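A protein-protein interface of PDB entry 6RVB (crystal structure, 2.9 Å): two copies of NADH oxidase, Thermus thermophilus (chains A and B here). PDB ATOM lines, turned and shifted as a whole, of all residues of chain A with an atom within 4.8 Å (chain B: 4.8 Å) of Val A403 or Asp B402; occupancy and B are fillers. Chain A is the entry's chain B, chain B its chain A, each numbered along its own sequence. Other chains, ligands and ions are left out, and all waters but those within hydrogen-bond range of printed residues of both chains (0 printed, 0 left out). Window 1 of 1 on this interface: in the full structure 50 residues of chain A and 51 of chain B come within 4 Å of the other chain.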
ATOM      1  N   ARG A 400      32.053  -5.259   4.581  1.00  0.00           N
ATOM      2  CA  ARG A 400      30.817  -5.747   5.130  1.00  0.00           C
ATOM      3  C   ARG A 400      30.326  -6.798   4.143  1.00  0.00           C
ATOM      4  O   ARG A 400      29.351  -7.451   4.400  1.00  0.00           O
ATOM      5  CB  ARG A 400      29.812  -4.601   5.160  1.00  0.00           C
ATOM      6  CG  ARG A 400      29.779  -3.792   6.405  1.00  0.00           C
ATOM      7  CD  ARG A 400      29.084  -2.461   6.295  1.00  0.00           C
ATOM      8  NE  ARG A 400      30.123  -1.439   6.289  1.00  0.00           N
ATOM      9  CZ  ARG A 400      30.259  -0.523   7.244  1.00  0.00           C
ATOM     10  NH1 ARG A 400      29.428  -0.455   8.275  1.00  0.00           N
ATOM     11  NH2 ARG A 400      31.227   0.350   7.143  1.00  0.00           N
ATOM     12  N   ILE A 401      30.952  -6.921   2.970  1.00  0.00           N
ATOM     13  CA  ILE A 401      30.491  -7.893   1.962  1.00  0.00           C
ATOM     14  C   ILE A 401      30.491  -9.248   2.547  1.00  0.00           C
ATOM     15  O   ILE A 401      29.631 -10.004   2.167  1.00  0.00           O
ATOM     16  CB  ILE A 401      31.399  -7.963   0.693  1.00  0.00           C
ATOM     17  CG1 ILE A 401      30.765  -8.808  -0.395  1.00  0.00           C
ATOM     18  CG2 ILE A 401      32.705  -8.460   1.007  1.00  0.00           C
ATOM     19  CD1 ILE A 401      29.583  -8.092  -0.968  1.00  0.00           C
ATOM     20  N   ASP A 402      31.470  -9.536   3.448  1.00  0.00           N
ATOM     21  CA  ASP A 402      31.586 -10.816   4.157  1.00  0.00           C
ATOM     22  C   ASP A 402      30.265 -11.200   4.918  1.00  0.00           C
ATOM     23  O   ASP A 402      29.966 -12.337   5.048  1.00  0.00           O
ATOM     24  CB  ASP A 402      32.810 -10.878   5.093  1.00  0.00           C
ATOM     25  CG  ASP A 402      34.099 -10.963   4.349  1.00  0.00           C
ATOM     26  OD1 ASP A 402      33.962 -11.268   3.181  1.00  0.00           O
ATOM     27  OD2 ASP A 402      35.263 -10.759   4.834  1.00  0.00           O
ATOM     28  N   VAL A 403      29.476 -10.260   5.418  1.00  0.00           N
ATOM     29  CA  VAL A 403      28.236 -10.574   6.087  1.00  0.00           C
ATOM     30  C   VAL A 403      27.273 -11.194   5.103  1.00  0.00           C
ATOM     31  O   VAL A 403      26.526 -12.093   5.456  1.00  0.00           O
ATOM     32  CB  VAL A 403      27.579  -9.315   6.714  1.00  0.00           C
ATOM     33  CG1 VAL A 403      26.188  -9.607   7.226  1.00  0.00           C
ATOM     34  CG2 VAL A 403      28.368  -8.953   7.887  1.00  0.00           C
ATOM     35  N   LEU A 404      27.280 -10.698   3.866  1.00  0.00           N
ATOM     36  CA  LEU A 404      26.325 -11.179   2.877  1.00  0.00           C
ATOM     37  C   LEU A 404      26.737 -12.547   2.412  1.00  0.00           C
ATOM     38  O   LEU A 404      25.873 -13.378   2.134  1.00  0.00           O
ATOM     39  CB  LEU A 404      26.195 -10.238   1.679  1.00  0.00           C
ATOM     40  CG  LEU A 404      25.760  -8.810   1.955  1.00  0.00           C
ATOM     41  CD1 LEU A 404      25.755  -8.095   0.662  1.00  0.00           C
ATOM     42  CD2 LEU A 404      24.383  -8.738   2.533  1.00  0.00           C
ATOM     43  N   ALA A 405      28.053 -12.775   2.312  1.00  0.00           N
ATOM     44  CA  ALA A 405      28.606 -14.086   1.970  1.00  0.00           C
ATOM     45  C   ALA A 405      28.203 -15.065   3.077  1.00  0.00           C
ATOM     46  O   ALA A 405      27.773 -16.169   2.813  1.00  0.00           O
ATOM     47  CB  ALA A 405      30.115 -14.034   1.742  1.00  0.00           C
ATOM     48  N   ALA A 406      28.263 -14.653   4.326  1.00  0.00           N
ATOM     49  CA  ALA A 406      27.822 -15.542   5.387  1.00  0.00           C
ATOM     50  C   ALA A 406      26.315 -15.943   5.215  1.00  0.00           C
ATOM     51  O   ALA A 406      25.938 -17.101   5.426  1.00  0.00           O
ATOM     52  CB  ALA A 406      28.075 -14.881   6.710  1.00  0.00           C
ATOM     53  N   LEU A 407      25.450 -14.977   4.889  1.00  0.00           N
ATOM     54  CA  LEU A 407      24.041 -15.236   4.681  1.00  0.00           C
ATOM     55  C   LEU A 407      23.791 -16.036   3.399  1.00  0.00           C
ATOM     56  O   LEU A 407      22.975 -16.929   3.394  1.00  0.00           O
ATOM     57  CB  LEU A 407      23.304 -13.941   4.614  1.00  0.00           C
ATOM     58  CG  LEU A 407      23.123 -13.162   5.902  1.00  0.00           C
ATOM     59  CD1 LEU A 407      22.590 -11.800   5.578  1.00  0.00           C
ATOM     60  CD2 LEU A 407      22.150 -13.883   6.665  1.00  0.00           C
ATOM     61  N   LEU A 417      18.929 -10.691   7.353  1.00  0.00           N
ATOM     62  CA  LEU A 417      19.872  -9.596   7.352  1.00  0.00           C
ATOM     63  C   LEU A 417      19.331  -8.506   8.204  1.00  0.00           C
ATOM     64  O   LEU A 417      20.048  -7.899   8.958  1.00  0.00           O
ATOM     65  CB  LEU A 417      20.093  -9.078   5.937  1.00  0.00           C
ATOM     66  CG  LEU A 417      20.971  -7.815   5.794  1.00  0.00           C
ATOM     67  CD1 LEU A 417      22.256  -7.916   6.569  1.00  0.00           C
ATOM     68  CD2 LEU A 417      21.274  -7.467   4.363  1.00  0.00           C
ATOM     69  N   LEU A 420      20.052  -8.863  12.081  1.00  0.00           N
ATOM     70  CA  LEU A 420      21.439  -8.905  12.531  1.00  0.00           C
ATOM     71  C   LEU A 420      21.738  -7.801  13.508  1.00  0.00           C
ATOM     72  O   LEU A 420      21.272  -6.681  13.351  1.00  0.00           O
ATOM     73  CB  LEU A 420      22.426  -8.876  11.369  1.00  0.00           C
ATOM     74  CG  LEU A 420      22.363 -10.162  10.552  1.00  0.00           C
ATOM     75  CD1 LEU A 420      23.636 -10.304   9.816  1.00  0.00           C
ATOM     76  CD2 LEU A 420      22.123 -11.368  11.386  1.00  0.00           C
ATOM     77  N   ASP A 421      22.486  -8.143  14.548  1.00  0.00           N
ATOM     78  CA  ASP A 421      23.001  -7.167  15.484  1.00  0.00           C
ATOM     79  C   ASP A 421      24.400  -6.681  15.084  1.00  0.00           C
ATOM     80  O   ASP A 421      25.400  -7.090  15.637  1.00  0.00           O
ATOM     81  CB  ASP A 421      23.083  -7.872  16.817  1.00  0.00           C
ATOM     82  CG  ASP A 421      23.465  -6.967  17.985  1.00  0.00           C
ATOM     83  OD1 ASP A 421      23.557  -5.704  17.815  1.00  0.00           O
ATOM     84  OD2 ASP A 421      23.645  -7.590  19.083  1.00  0.00           O
ATOM     85  N   LEU A 422      24.482  -5.769  14.134  1.00  0.00           N
ATOM     86  CA  LEU A 422      25.787  -5.316  13.688  1.00  0.00           C
ATOM     87  C   LEU A 422      26.474  -4.323  14.612  1.00  0.00           C
ATOM     88  O   LEU A 422      25.865  -3.808  15.532  1.00  0.00           O
ATOM     89  CB  LEU A 422      25.651  -4.720  12.318  1.00  0.00           C
ATOM     90  CG  LEU A 422      24.970  -5.627  11.367  1.00  0.00           C
ATOM     91  CD1 LEU A 422      24.999  -4.861  10.078  1.00  0.00           C
ATOM     92  CD2 LEU A 422      25.698  -6.915  11.346  1.00  0.00           C
ATOM     93  N   ALA A 423      27.751  -4.069  14.327  1.00  0.00           N
ATOM     94  CA  ALA A 423      28.528  -3.098  15.096  1.00  0.00           C
ATOM     95  C   ALA A 423      28.371  -1.664  14.614  1.00  0.00           C
ATOM     96  O   ALA A 423      28.411  -1.405  13.367  1.00  0.00           O
ATOM     97  CB  ALA A 423      29.901  -3.437  15.011  1.00  0.00           C
ATOM     98  N   ASP A 433      23.456   0.453  10.119  1.00  0.00           N
ATOM     99  CA  ASP A 433      24.539   0.080   9.219  1.00  0.00           C
ATOM    100  C   ASP A 433      24.073   0.100   7.730  1.00  0.00           C
ATOM    101  O   ASP A 433      22.940  -0.286   7.407  1.00  0.00           O
ATOM    102  CB  ASP A 433      25.054  -1.270   9.614  1.00  0.00           C
ATOM    103  CG  ASP A 433      26.205  -1.718   8.764  1.00  0.00           C
ATOM    104  OD1 ASP A 433      25.952  -2.240   7.638  1.00  0.00           O
ATOM    105  OD2 ASP A 433      27.372  -1.585   9.237  1.00  0.00           O
ATOM    106  N   LEU A 435      24.311  -1.998   5.495  1.00  0.00           N
ATOM    107  CA  LEU A 435      23.603  -3.235   5.209  1.00  0.00           C
ATOM    108  C   LEU A 435      22.150  -3.168   5.707  1.00  0.00           C
ATOM    109  O   LEU A 435      21.288  -3.679   5.066  1.00  0.00           O
ATOM    110  CB  LEU A 435      24.319  -4.455   5.792  1.00  0.00           C
ATOM    111  CG  LEU A 435      25.679  -4.627   5.184  1.00  0.00           C
ATOM    112  CD1 LEU A 435      26.490  -5.540   6.040  1.00  0.00           C
ATOM    113  CD2 LEU A 435      25.547  -5.183   3.846  1.00  0.00           C
ATOM    114  N   THR B 326      26.982  -7.351  20.091  1.00  0.00           N
ATOM    115  CA  THR B 326      28.054  -6.757  19.276  1.00  0.00           C
ATOM    116  C   THR B 326      28.380  -5.337  19.687  1.00  0.00           C
ATOM    117  O   THR B 326      27.455  -4.564  19.852  1.00  0.00           O
ATOM    118  CB  THR B 326      27.687  -6.775  17.797  1.00  0.00           C
ATOM    119  OG1 THR B 326      27.186  -8.078  17.446  1.00  0.00           O
ATOM    120  CG2 THR B 326      28.797  -6.389  16.955  1.00  0.00           C
ATOM    121  N   LEU B 399      35.740  -5.387  12.584  1.00  0.00           N
ATOM    122  CA  LEU B 399      34.487  -4.980  11.720  1.00  0.00           C
ATOM    123  C   LEU B 399      34.119  -6.203  10.882  1.00  0.00           C
ATOM    124  O   LEU B 399      32.983  -6.323  10.421  1.00  0.00           O
ATOM    125  CB  LEU B 399      34.545  -3.815  10.587  1.00  0.00           C
ATOM    126  CG  LEU B 399      33.167  -3.110  10.478  1.00  0.00           C
ATOM    127  CD1 LEU B 399      32.605  -2.464  11.825  1.00  0.00           C
ATOM    128  CD2 LEU B 399      33.094  -1.929   9.612  1.00  0.00           C
ATOM    129  N   ARG B 400      35.124  -7.052  10.629  1.00  0.00           N
ATOM    130  CA  ARG B 400      34.888  -8.467  10.464  1.00  0.00           C
ATOM    131  C   ARG B 400      34.009  -9.021  11.656  1.00  0.00           C
ATOM    132  O   ARG B 400      33.337 -10.007  11.531  1.00  0.00           O
ATOM    133  CB  ARG B 400      36.218  -9.208  10.360  1.00  0.00           C
ATOM    134  CG  ARG B 400      36.775  -9.381   8.994  1.00  0.00           C
ATOM    135  CD  ARG B 400      38.192  -9.863   8.981  1.00  0.00           C
ATOM    136  NE  ARG B 400      39.029  -8.705   8.779  1.00  0.00           N
ATOM    137  CZ  ARG B 400      39.794  -8.525   7.718  1.00  0.00           C
ATOM    138  NH1 ARG B 400      39.864  -9.438   6.779  1.00  0.00           N
ATOM    139  NH2 ARG B 400      40.505  -7.413   7.614  1.00  0.00           N
ATOM    140  N   ILE B 401      33.983  -8.354  12.800  1.00  0.00           N
ATOM    141  CA  ILE B 401      33.144  -8.799  13.884  1.00  0.00           C
ATOM    142  C   ILE B 401      31.731  -9.049  13.385  1.00  0.00           C
ATOM    143  O   ILE B 401      31.065  -9.939  13.890  1.00  0.00           O
ATOM    144  CB  ILE B 401      33.082  -7.760  15.016  1.00  0.00           C
ATOM    145  CG1 ILE B 401      32.565  -8.397  16.286  1.00  0.00           C
ATOM    146  CG2 ILE B 401      32.162  -6.694  14.703  1.00  0.00           C
ATOM    147  CD1 ILE B 401      33.505  -9.227  16.928  1.00  0.00           C
ATOM    148  N   ASP B 402      31.272  -8.290  12.389  1.00  0.00           N
ATOM    149  CA  ASP B 402      29.912  -8.441  11.900  1.00  0.00           C
ATOM    150  C   ASP B 402      29.666  -9.878  11.425  1.00  0.00           C
ATOM    151  O   ASP B 402      28.586 -10.408  11.585  1.00  0.00           O
ATOM    152  CB  ASP B 402      29.553  -7.370  10.829  1.00  0.00           C
ATOM    153  CG  ASP B 402      29.204  -6.035  11.443  1.00  0.00           C
ATOM    154  OD1 ASP B 402      28.932  -6.026  12.688  1.00  0.00           O
ATOM    155  OD2 ASP B 402      29.201  -4.958  10.742  1.00  0.00           O
ATOM    156  N   VAL B 403      30.688 -10.531  10.874  1.00  0.00           N
ATOM    157  CA  VAL B 403      30.543 -11.877  10.414  1.00  0.00           C
ATOM    158  C   VAL B 403      30.142 -12.801  11.556  1.00  0.00           C
ATOM    159  O   VAL B 403      29.209 -13.594  11.435  1.00  0.00           O
ATOM    160  CB  VAL B 403      31.798 -12.422   9.739  1.00  0.00           C
ATOM    161  CG1 VAL B 403      31.573 -13.919   9.392  1.00  0.00           C
ATOM    162  CG2 VAL B 403      31.979 -11.701   8.450  1.00  0.00           C
ATOM    163  N   LEU B 404      30.823 -12.674  12.688  1.00  0.00           N
ATOM    164  CA  LEU B 404      30.569 -13.551  13.793  1.00  0.00           C
ATOM    165  C   LEU B 404      29.229 -13.249  14.362  1.00  0.00           C
ATOM    166  O   LEU B 404      28.541 -14.177  14.756  1.00  0.00           O
ATOM    167  CB  LEU B 404      31.630 -13.392  14.847  1.00  0.00           C
ATOM    168  CG  LEU B 404      33.083 -13.598  14.473  1.00  0.00           C
ATOM    169  CD1 LEU B 404      33.888 -13.137  15.686  1.00  0.00           C
ATOM    170  CD2 LEU B 404      33.260 -15.036  14.173  1.00  0.00           C
ATOM    171  N   ALA B 405      28.827 -11.981  14.400  1.00  0.00           N
ATOM    172  CA  ALA B 405      27.462 -11.692  14.794  1.00  0.00           C
ATOM    173  C   ALA B 405      26.475 -12.361  13.858  1.00  0.00           C
ATOM    174  O   ALA B 405      25.480 -12.913  14.320  1.00  0.00           O
ATOM    175  CB  ALA B 405      27.200 -10.266  14.878  1.00  0.00           C
ATOM    176  N   ALA B 406      26.720 -12.385  12.556  1.00  0.00           N
ATOM    177  CA  ALA B 406      25.802 -13.157  11.687  1.00  0.00           C
ATOM    178  C   ALA B 406      25.684 -14.642  12.106  1.00  0.00           C
ATOM    179  O   ALA B 406      24.613 -15.202  12.129  1.00  0.00           O
ATOM    180  CB  ALA B 406      26.206 -13.067  10.327  1.00  0.00           C
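Of the printed residues of chain B, Val A403 touches Asp B402 (3.5 Å). Asp B402 touches three residues of chain A. Of the printed residues of chain A, Ile B401 touches Ala A423. Of the printed residues of chain A, Val B403 touches Asp A402 (3.6 Å). Of the printed residues of chain B, Arg A400 touches Leu B399. Printed residues of chain B within 4 Å of Leu A420: Ala B406. The nearest residue of chain B that does not touch Val A403 is Val B403 (4.1 Å). The nearest printed residue of chain A that does not touch Thr B326 is Leu A420 (6.7 Å).
The guanidinium group (NH1) of Arg A400 lies within salt-bridge range of the side-chain carboxylate (OD2) of Asp A433 (2.5 Å).
Asp A402 touches Val B403, and with the chains exchanged Val A403 touches Asp B402. Positions printed for both chains: 400, 401, 402, 403, 404, 405 and 406. Of the 11 pairs that touch across the chains among the printed residues, 2 have their exchanged pair printed and touching as well.
Among the printed residues, merely in contact across the chains: Arg A400 with Leu B399 (3.8 Å), Asp A402 with Val B403 (3.6 Å), Val A403 with Asp B402 (3.5 Å), Leu A420 with Ala B406 (3.8 Å), Asp A421 with Ala B405 (3.7 Å), Leu A422 with Thr B326 (3.9 Å), Leu A422 with Asp B402 (3.4 Å), Ala A423 with Thr B326 (3.7 Å) and Ala A423 with Ile B401 (3.98 Å).
Of the 9 printed residues of chain B, 7 touch a printed residue of chain A. Printed residues of chain B that touch a printed residue of chain A: Thr B326, Leu B399, Ile B401, Asp B402, Val B403, Ala B405 and Ala B406. Hydrophobic or aromatic side chains of chain B that line the printed part of chain A: Leu B399, Ile B401, Val B403, Ala B405 and Ala B406. Hydrophobic or aromatic side chains of chain A that line the printed part of chain B: Val A403, Leu A420, Leu A422 and Ala A423. Among the printed residues, 11 pairs touch across the chains. Among the printed residues, no Asp or Glu carboxylate lies within 4 Å of a Lys or Arg side-chain nitrogen of the other chain.
N of Ala A423 is in hydrogen-bond range of OD1 of Asp B402 (2.8 Å). The side-chain hydroxyl of Thr B326 is in hydrogen-bond range of the backbone carbonyl oxygen of Asp A421 (2.7 Å).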
